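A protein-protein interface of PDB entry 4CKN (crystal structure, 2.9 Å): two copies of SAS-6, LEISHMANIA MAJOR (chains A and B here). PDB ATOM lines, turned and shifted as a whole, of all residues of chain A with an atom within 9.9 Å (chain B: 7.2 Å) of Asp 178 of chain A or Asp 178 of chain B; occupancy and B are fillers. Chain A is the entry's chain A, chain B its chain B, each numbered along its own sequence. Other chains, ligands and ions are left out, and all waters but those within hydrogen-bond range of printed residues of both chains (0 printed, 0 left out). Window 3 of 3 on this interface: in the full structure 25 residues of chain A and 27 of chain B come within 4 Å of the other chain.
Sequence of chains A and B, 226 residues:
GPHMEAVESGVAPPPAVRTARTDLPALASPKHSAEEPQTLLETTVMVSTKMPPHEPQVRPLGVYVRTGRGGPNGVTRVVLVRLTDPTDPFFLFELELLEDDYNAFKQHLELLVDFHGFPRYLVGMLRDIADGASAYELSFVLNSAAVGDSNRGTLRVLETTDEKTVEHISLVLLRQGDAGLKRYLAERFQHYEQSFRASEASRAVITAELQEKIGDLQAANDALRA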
ATOM      1  N   PRO A  89      25.473 -24.451 -25.936  1.00  0.00           N
ATOM      2  CA  PRO A  89      24.045 -24.417 -26.193  1.00  0.00           C
ATOM      3  C   PRO A  89      23.173 -24.937 -25.054  1.00  0.00           C
ATOM      4  O   PRO A  89      21.956 -24.743 -25.101  1.00  0.00           O
ATOM      5  CB  PRO A  89      23.887 -25.335 -27.406  1.00  0.00           C
ATOM      6  CG  PRO A  89      25.230 -25.393 -28.035  1.00  0.00           C
ATOM      7  CD  PRO A  89      26.187 -25.305 -26.898  1.00  0.00           C
ATOM      8  N   PHE A  90      23.756 -25.627 -24.076  1.00  0.00           N
ATOM      9  CA  PHE A  90      22.973 -26.143 -22.944  1.00  0.00           C
ATOM     10  C   PHE A  90      22.937 -25.164 -21.799  1.00  0.00           C
ATOM     11  O   PHE A  90      22.205 -25.346 -20.832  1.00  0.00           O
ATOM     12  CB  PHE A  90      23.522 -27.475 -22.443  1.00  0.00           C
ATOM     13  CG  PHE A  90      23.142 -28.657 -23.271  1.00  0.00           C
ATOM     14  CD1 PHE A  90      22.473 -28.539 -24.484  1.00  0.00           C
ATOM     15  CD2 PHE A  90      23.449 -29.913 -22.800  1.00  0.00           C
ATOM     16  CE1 PHE A  90      22.136 -29.668 -25.202  1.00  0.00           C
ATOM     17  CE2 PHE A  90      23.116 -31.041 -23.509  1.00  0.00           C
ATOM     18  CZ  PHE A  90      22.458 -30.923 -24.713  1.00  0.00           C
ATOM     19  N   LEU A  92      21.461 -22.116 -20.429  1.00  0.00           N
ATOM     20  CA  LEU A  92      20.299 -21.241 -20.600  1.00  0.00           C
ATOM     21  C   LEU A  92      19.708 -20.810 -19.255  1.00  0.00           C
ATOM     22  O   LEU A  92      19.202 -21.631 -18.496  1.00  0.00           O
ATOM     23  CB  LEU A  92      19.214 -21.940 -21.415  1.00  0.00           C
ATOM     24  CG  LEU A  92      17.933 -21.123 -21.628  1.00  0.00           C
ATOM     25  CD1 LEU A  92      18.184 -19.995 -22.616  1.00  0.00           C
ATOM     26  CD2 LEU A  92      16.786 -22.012 -22.092  1.00  0.00           C
ATOM     27  N   ARG A 175      18.160 -21.370 -14.051  1.00  0.00           N
ATOM     28  CA  ARG A 175      18.536 -22.305 -15.104  1.00  0.00           C
ATOM     29  C   ARG A 175      17.267 -22.994 -15.539  1.00  0.00           C
ATOM     30  O   ARG A 175      16.425 -23.324 -14.709  1.00  0.00           O
ATOM     31  CB  ARG A 175      19.553 -23.346 -14.623  1.00  0.00           C
ATOM     32  CG  ARG A 175      19.734 -24.509 -15.585  1.00  0.00           C
ATOM     33  CD  ARG A 175      20.675 -25.548 -15.020  1.00  0.00           C
ATOM     34  NE  ARG A 175      22.013 -24.985 -14.975  1.00  0.00           N
ATOM     35  CZ  ARG A 175      22.962 -25.333 -14.113  1.00  0.00           C
ATOM     36  NH1 ARG A 175      22.741 -26.252 -13.174  1.00  0.00           N
ATOM     37  NH2 ARG A 175      24.142 -24.737 -14.180  1.00  0.00           N
ATOM     38  N   GLN A 176      17.138 -23.207 -16.839  1.00  0.00           N
ATOM     39  CA  GLN A 176      15.937 -23.785 -17.385  1.00  0.00           C
ATOM     40  C   GLN A 176      16.048 -25.289 -17.516  1.00  0.00           C
ATOM     41  O   GLN A 176      17.123 -25.832 -17.779  1.00  0.00           O
ATOM     42  CB  GLN A 176      15.631 -23.136 -18.725  1.00  0.00           C
ATOM     43  CG  GLN A 176      15.126 -21.707 -18.538  1.00  0.00           C
ATOM     44  CD  GLN A 176      13.642 -21.672 -18.146  1.00  0.00           C
ATOM     45  OE1 GLN A 176      13.282 -21.186 -17.068  1.00  0.00           O
ATOM     46  NE2 GLN A 176      12.788 -22.244 -18.981  1.00  0.00           N
ATOM     47  N   GLY A 177      14.911 -25.956 -17.340  1.00  0.00           N
ATOM     48  CA  GLY A 177      14.856 -27.409 -17.397  1.00  0.00           C
ATOM     49  C   GLY A 177      14.818 -27.899 -18.832  1.00  0.00           C
ATOM     50  O   GLY A 177      14.627 -27.112 -19.768  1.00  0.00           O
ATOM     51  N   ASP A 178      15.012 -29.203 -18.998  1.00  0.00           N
ATOM     52  CA  ASP A 178      15.021 -29.835 -20.313  1.00  0.00           C
ATOM     53  C   ASP A 178      13.889 -29.332 -21.194  1.00  0.00           C
ATOM     54  O   ASP A 178      14.107 -28.992 -22.345  1.00  0.00           O
ATOM     55  CB  ASP A 178      14.936 -31.356 -20.169  1.00  0.00           C
ATOM     56  CG  ASP A 178      16.262 -31.984 -19.766  1.00  0.00           C
ATOM     57  OD1 ASP A 178      17.187 -31.238 -19.383  1.00  0.00           O
ATOM     58  OD2 ASP A 178      16.387 -33.229 -19.836  1.00  0.00           O
ATOM     59  N   ALA A 179      12.686 -29.256 -20.644  1.00  0.00           N
ATOM     60  CA  ALA A 179      11.535 -28.776 -21.405  1.00  0.00           C
ATOM     61  C   ALA A 179      11.835 -27.426 -22.063  1.00  0.00           C
ATOM     62  O   ALA A 179      11.813 -27.306 -23.279  1.00  0.00           O
ATOM     63  CB  ALA A 179      10.311 -28.669 -20.503  1.00  0.00           C
ATOM     64  N   GLY A 180      12.131 -26.419 -21.246  1.00  0.00           N
ATOM     65  CA  GLY A 180      12.405 -25.063 -21.726  1.00  0.00           C
ATOM     66  C   GLY A 180      13.663 -24.940 -22.567  1.00  0.00           C
ATOM     67  O   GLY A 180      13.773 -24.073 -23.435  1.00  0.00           O
ATOM     68  N   LEU A 181      14.623 -25.812 -22.294  1.00  0.00           N
ATOM     69  CA  LEU A 181      15.866 -25.838 -23.046  1.00  0.00           C
ATOM     70  C   LEU A 181      15.634 -26.417 -24.437  1.00  0.00           C
ATOM     71  O   LEU A 181      16.112 -25.862 -25.422  1.00  0.00           O
ATOM     72  CB  LEU A 181      16.892 -26.675 -22.298  1.00  0.00           C
ATOM     73  CG  LEU A 181      18.291 -26.768 -22.877  1.00  0.00           C
ATOM     74  CD1 LEU A 181      18.937 -25.404 -22.999  1.00  0.00           C
ATOM     75  CD2 LEU A 181      19.123 -27.661 -21.974  1.00  0.00           C
ATOM     76  N   LYS A 182      14.901 -27.527 -24.507  1.00  0.00           N
ATOM     77  CA  LYS A 182      14.564 -28.147 -25.779  1.00  0.00           C
ATOM     78  C   LYS A 182      13.835 -27.148 -26.656  1.00  0.00           C
ATOM     79  O   LYS A 182      14.172 -26.965 -27.815  1.00  0.00           O
ATOM     80  CB  LYS A 182      13.687 -29.385 -25.577  1.00  0.00           C
ATOM     81  CG  LYS A 182      14.429 -30.605 -25.052  1.00  0.00           C
ATOM     82  CD  LYS A 182      13.585 -31.874 -25.120  1.00  0.00           C
ATOM     83  CE  LYS A 182      12.412 -31.858 -24.154  1.00  0.00           C
ATOM     84  NZ  LYS A 182      11.406 -32.894 -24.518  1.00  0.00           N
ATOM     85  N   ARG A 183      12.818 -26.515 -26.091  1.00  0.00           N
ATOM     86  CA  ARG A 183      12.085 -25.451 -26.768  1.00  0.00           C
ATOM     87  C   ARG A 183      13.029 -24.388 -27.309  1.00  0.00           C
ATOM     88  O   ARG A 183      12.938 -24.016 -28.474  1.00  0.00           O
ATOM     89  CB  ARG A 183      11.059 -24.819 -25.814  1.00  0.00           C
ATOM     90  CG  ARG A 183       9.620 -25.221 -26.119  1.00  0.00           C
ATOM     91  CD  ARG A 183       8.582 -24.681 -25.162  1.00  0.00           C
ATOM     92  NE  ARG A 183       8.532 -25.338 -23.837  1.00  0.00           N
ATOM     93  CZ  ARG A 183       8.872 -24.775 -22.672  1.00  0.00           C
ATOM     94  NH1 ARG A 183       9.316 -23.520 -22.617  1.00  0.00           N
ATOM     95  NH2 ARG A 183       8.771 -25.478 -21.541  1.00  0.00           N
ATOM     96  N   TYR A 184      13.940 -23.914 -26.464  1.00  0.00           N
ATOM     97  CA  TYR A 184      14.912 -22.903 -26.876  1.00  0.00           C
ATOM     98  C   TYR A 184      15.717 -23.426 -28.063  1.00  0.00           C
ATOM     99  O   TYR A 184      15.774 -22.797 -29.127  1.00  0.00           O
ATOM    100  CB  TYR A 184      15.829 -22.513 -25.707  1.00  0.00           C
ATOM    101  CG  TYR A 184      17.031 -21.728 -26.115  1.00  0.00           C
ATOM    102  CD1 TYR A 184      16.896 -20.420 -26.597  1.00  0.00           C
ATOM    103  CD2 TYR A 184      18.317 -22.275 -26.014  1.00  0.00           C
ATOM    104  CE1 TYR A 184      18.012 -19.688 -26.981  1.00  0.00           C
ATOM    105  CE2 TYR A 184      19.444 -21.541 -26.390  1.00  0.00           C
ATOM    106  CZ  TYR A 184      19.280 -20.246 -26.878  1.00  0.00           C
ATOM    107  OH  TYR A 184      20.361 -19.482 -27.277  1.00  0.00           O
ATOM    108  N   LEU A 185      16.316 -24.594 -27.877  1.00  0.00           N
ATOM    109  CA  LEU A 185      17.157 -25.193 -28.906  1.00  0.00           C
ATOM    110  C   LEU A 185      16.411 -25.410 -30.194  1.00  0.00           C
ATOM    111  O   LEU A 185      16.915 -25.101 -31.262  1.00  0.00           O
ATOM    112  CB  LEU A 185      17.727 -26.514 -28.434  1.00  0.00           C
ATOM    113  CG  LEU A 185      18.769 -26.357 -27.331  1.00  0.00           C
ATOM    114  CD1 LEU A 185      19.092 -27.710 -26.728  1.00  0.00           C
ATOM    115  CD2 LEU A 185      20.024 -25.699 -27.872  1.00  0.00           C
ATOM    116  N   ALA A 186      15.195 -25.912 -30.085  1.00  0.00           N
ATOM    117  CA  ALA A 186      14.367 -26.098 -31.251  1.00  0.00           C
ATOM    118  C   ALA A 186      14.196 -24.764 -31.969  1.00  0.00           C
ATOM    119  O   ALA A 186      14.560 -24.628 -33.127  1.00  0.00           O
ATOM    120  CB  ALA A 186      13.015 -26.666 -30.853  1.00  0.00           C
ATOM    121  N   GLN B 176      14.659 -41.319 -29.412  1.00  0.00           N
ATOM    122  CA  GLN B 176      15.716 -40.917 -28.512  1.00  0.00           C
ATOM    123  C   GLN B 176      15.213 -40.039 -27.380  1.00  0.00           C
ATOM    124  O   GLN B 176      14.217 -39.302 -27.505  1.00  0.00           O
ATOM    125  CB  GLN B 176      16.885 -40.310 -29.256  1.00  0.00           C
ATOM    126  CG  GLN B 176      18.056 -41.256 -29.340  1.00  0.00           C
ATOM    127  CD  GLN B 176      19.253 -40.608 -29.956  1.00  0.00           C
ATOM    128  OE1 GLN B 176      19.140 -39.991 -31.009  1.00  0.00           O
ATOM    129  NE2 GLN B 176      20.410 -40.717 -29.300  1.00  0.00           N
ATOM    130  N   GLY B 177      15.915 -40.157 -26.260  1.00  0.00           N
ATOM    131  CA  GLY B 177      15.547 -39.462 -25.052  1.00  0.00           C
ATOM    132  C   GLY B 177      16.023 -38.026 -25.086  1.00  0.00           C
ATOM    133  O   GLY B 177      16.811 -37.631 -25.957  1.00  0.00           O
ATOM    134  N   ASP B 178      15.534 -37.241 -24.132  1.00  0.00           N
ATOM    135  CA  ASP B 178      15.888 -35.833 -24.022  1.00  0.00           C
ATOM    136  C   ASP B 178      17.382 -35.597 -24.223  1.00  0.00           C
ATOM    137  O   ASP B 178      17.768 -34.709 -24.975  1.00  0.00           O
ATOM    138  CB  ASP B 178      15.451 -35.285 -22.661  1.00  0.00           C
ATOM    139  CG  ASP B 178      13.954 -34.995 -22.594  1.00  0.00           C
ATOM    140  OD1 ASP B 178      13.219 -35.429 -23.508  1.00  0.00           O
ATOM    141  OD2 ASP B 178      13.517 -34.326 -21.628  1.00  0.00           O
ATOM    142  N   ALA B 179      18.218 -36.403 -23.583  1.00  0.00           N
ATOM    143  CA  ALA B 179      19.671 -36.264 -23.726  1.00  0.00           C
ATOM    144  C   ALA B 179      20.101 -36.240 -25.199  1.00  0.00           C
ATOM    145  O   ALA B 179      20.644 -35.249 -25.677  1.00  0.00           O
ATOM    146  CB  ALA B 179      20.384 -37.386 -22.989  1.00  0.00           C
ATOM    147  N   GLY B 180      19.806 -37.318 -25.918  1.00  0.00           N
ATOM    148  CA  GLY B 180      20.155 -37.448 -27.327  1.00  0.00           C
ATOM    149  C   GLY B 180      19.447 -36.461 -28.235  1.00  0.00           C
ATOM    150  O   GLY B 180      19.967 -36.075 -29.291  1.00  0.00           O
ATOM    151  N   LEU B 181      18.249 -36.061 -27.841  1.00  0.00           N
ATOM    152  CA  LEU B 181      17.478 -35.097 -28.609  1.00  0.00           C
ATOM    153  C   LEU B 181      18.067 -33.700 -28.469  1.00  0.00           C
ATOM    154  O   LEU B 181      18.220 -32.979 -29.457  1.00  0.00           O
ATOM    155  CB  LEU B 181      16.032 -35.106 -28.130  1.00  0.00           C
ATOM    156  CG  LEU B 181      15.023 -34.221 -28.860  1.00  0.00           C
ATOM    157  CD1 LEU B 181      14.932 -34.577 -30.329  1.00  0.00           C
ATOM    158  CD2 LEU B 181      13.667 -34.376 -28.199  1.00  0.00           C
ATOM    159  N   LYS B 182      18.402 -33.324 -27.239  1.00  0.00           N
ATOM    160  CA  LYS B 182      19.033 -32.029 -26.972  1.00  0.00           C
ATOM    161  C   LYS B 182      20.330 -31.906 -27.765  1.00  0.00           C
ATOM    162  O   LYS B 182      20.556 -30.915 -28.446  1.00  0.00           O
ATOM    163  CB  LYS B 182      19.326 -31.859 -25.479  1.00  0.00           C
ATOM    164  CG  LYS B 182      18.102 -31.575 -24.614  1.00  0.00           C
ATOM    165  CD  LYS B 182      18.483 -31.157 -23.202  1.00  0.00           C
ATOM    166  CE  LYS B 182      19.120 -32.285 -22.402  1.00  0.00           C
ATOM    167  NZ  LYS B 182      19.839 -31.756 -21.210  1.00  0.00           N
ATOM    168  N   ARG B 183      21.171 -32.928 -27.667  1.00  0.00           N
ATOM    169  CA  ARG B 183      22.393 -33.021 -28.472  1.00  0.00           C
ATOM    170  C   ARG B 183      22.112 -32.800 -29.956  1.00  0.00           C
ATOM    171  O   ARG B 183      22.767 -31.996 -30.604  1.00  0.00           O
ATOM    172  CB  ARG B 183      23.080 -34.380 -28.253  1.00  0.00           C
ATOM    173  CG  ARG B 183      24.311 -34.304 -27.348  1.00  0.00           C
ATOM    174  CD  ARG B 183      24.416 -35.494 -26.393  1.00  0.00           C
ATOM    175  NE  ARG B 183      23.941 -36.755 -26.960  1.00  0.00           N
ATOM    176  CZ  ARG B 183      23.612 -37.831 -26.242  1.00  0.00           C
ATOM    177  NH1 ARG B 183      23.713 -37.832 -24.914  1.00  0.00           N
ATOM    178  NH2 ARG B 183      23.178 -38.919 -26.863  1.00  0.00           N
ATOM    179  N   TYR B 184      21.120 -33.500 -30.482  1.00  0.00           N
ATOM    180  CA  TYR B 184      20.745 -33.352 -31.883  1.00  0.00           C
ATOM    181  C   TYR B 184      20.367 -31.904 -32.168  1.00  0.00           C
ATOM    182  O   TYR B 184      20.929 -31.254 -33.059  1.00  0.00           O
ATOM    183  CB  TYR B 184      19.584 -34.306 -32.242  1.00  0.00           C
ATOM    184  CG  TYR B 184      18.933 -34.007 -33.571  1.00  0.00           C
ATOM    185  CD1 TYR B 184      19.626 -34.202 -34.759  1.00  0.00           C
ATOM    186  CD2 TYR B 184      17.632 -33.531 -33.641  1.00  0.00           C
ATOM    187  CE1 TYR B 184      19.043 -33.926 -35.987  1.00  0.00           C
ATOM    188  CE2 TYR B 184      17.035 -33.254 -34.871  1.00  0.00           C
ATOM    189  CZ  TYR B 184      17.748 -33.453 -36.046  1.00  0.00           C
ATOM    190  OH  TYR B 184      17.203 -33.191 -37.295  1.00  0.00           O
ATOM    191  N   LEU B 185      19.427 -31.396 -31.385  1.00  0.00           N
ATOM    192  CA  LEU B 185      18.942 -30.041 -31.576  1.00  0.00           C
ATOM    193  C   LEU B 185      20.067 -29.027 -31.475  1.00  0.00           C
ATOM    194  O   LEU B 185      20.143 -28.095 -32.271  1.00  0.00           O
ATOM    195  CB  LEU B 185      17.851 -29.714 -30.568  1.00  0.00           C
ATOM    196  CG  LEU B 185      16.548 -30.466 -30.823  1.00  0.00           C
ATOM    197  CD1 LEU B 185      15.616 -30.300 -29.633  1.00  0.00           C
ATOM    198  CD2 LEU B 185      15.880 -29.988 -32.102  1.00  0.00           C
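Of the 15 printed residues of chain A, 5 touch a printed residue of chain B.
Printed residues of chain A that touch a printed residue of chain B: Phe 90, Asp 178, Leu 181, Lys 182 and Leu 185.
Of the 10 printed residues of chain B, 5 touch a printed residue of chain A.
Among the printed residues, 10 pairs touch across the chains.
Among the printed residues, Asp or Glu carboxylates within 4 Å of a Lys or Arg side-chain nitrogen of the other chain: Asp 178 of chain A with Lys 182 of chain B (3.3 Å) and Lys 182 of chain A with Asp 178 of chain B (3.3 Å).
Asp 178 of chain A touches its own counterpart, Asp 178 of chain B.
Leu 181 of chain A touches Lys 182 of chain B, and with the chains exchanged Lys 182 of chain A touches Leu 181 of chain B.
Leu 185 of chain A touches Lys 182 of chain B, but with the chains exchanged Lys 182 of chain A does not touch Leu 185 of chain B (4.1 Å).
Leu 185 of chain A touches its own counterpart, Leu 185 of chain B.
Positions printed for both chains: 176, 177, 178, 179, 180, 181, 182, 183, 184 and 185.
Of the 10 pairs that touch across the chains among the printed residues, 7 have their exchanged pair printed and touching as well.
NZ of Lys 182 of chain A lies within salt-bridge range of OD1 of Asp 178 of chain B, 3.3 Å away.
NZ of Lys 182 of chain B is in salt-bridge range of OD1 of Asp 178 of chain A.
Lys 182 of chain B touches Phe 90 of chain A.
Phe 90 of chain A touches Arg 183 of chain B (CZ to N, 3.8 Å).
Asp 178 of chain A touches Asp 178 of chain B.
Leu 181 of chain A touches Lys 182 of chain B.
Leu 181 of chain B touches Lys 182 of chain A (CD2 to CD, 3.97 Å).
Lys 182 of chain A touches Lys 182 of chain B (CG to CG, 3.8 Å).
O of Lys 182 of chain B touches CD1 of Leu 185 of chain A, at 3.9 Å.
CB of Leu 185 of chain A touches CB of Leu 185 of chain B (3.8 Å).
Of chain B, only Asp 178 and Lys 182 come within 4 Å of Asp 178 of chain A.
Of the printed residues of chain B, Leu 181 of chain A touches Lys 182 (3.8 Å).
Of the printed residues of chain B, Leu 185 of chain A touches Lys 182 and Leu 185.
No residue of chain A comes within 4 Å of Gly 177 of chain B.
Of chain A, only Asp 178 and Lys 182 come within 4 Å of Asp 178 of chain B.
Lys 182 of chain B touches just these residues of chain A: Phe 90, Asp 178, Leu 181, Lys 182 and Leu 185.
The nearest residue of chain A that does not touch Asp 178 of chain B is Ala 179 of chain A (5.2 Å).
The nearest printed residue of chain B that does not touch Phe 90 of chain A is Ala 179 of chain B (4.8 Å).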
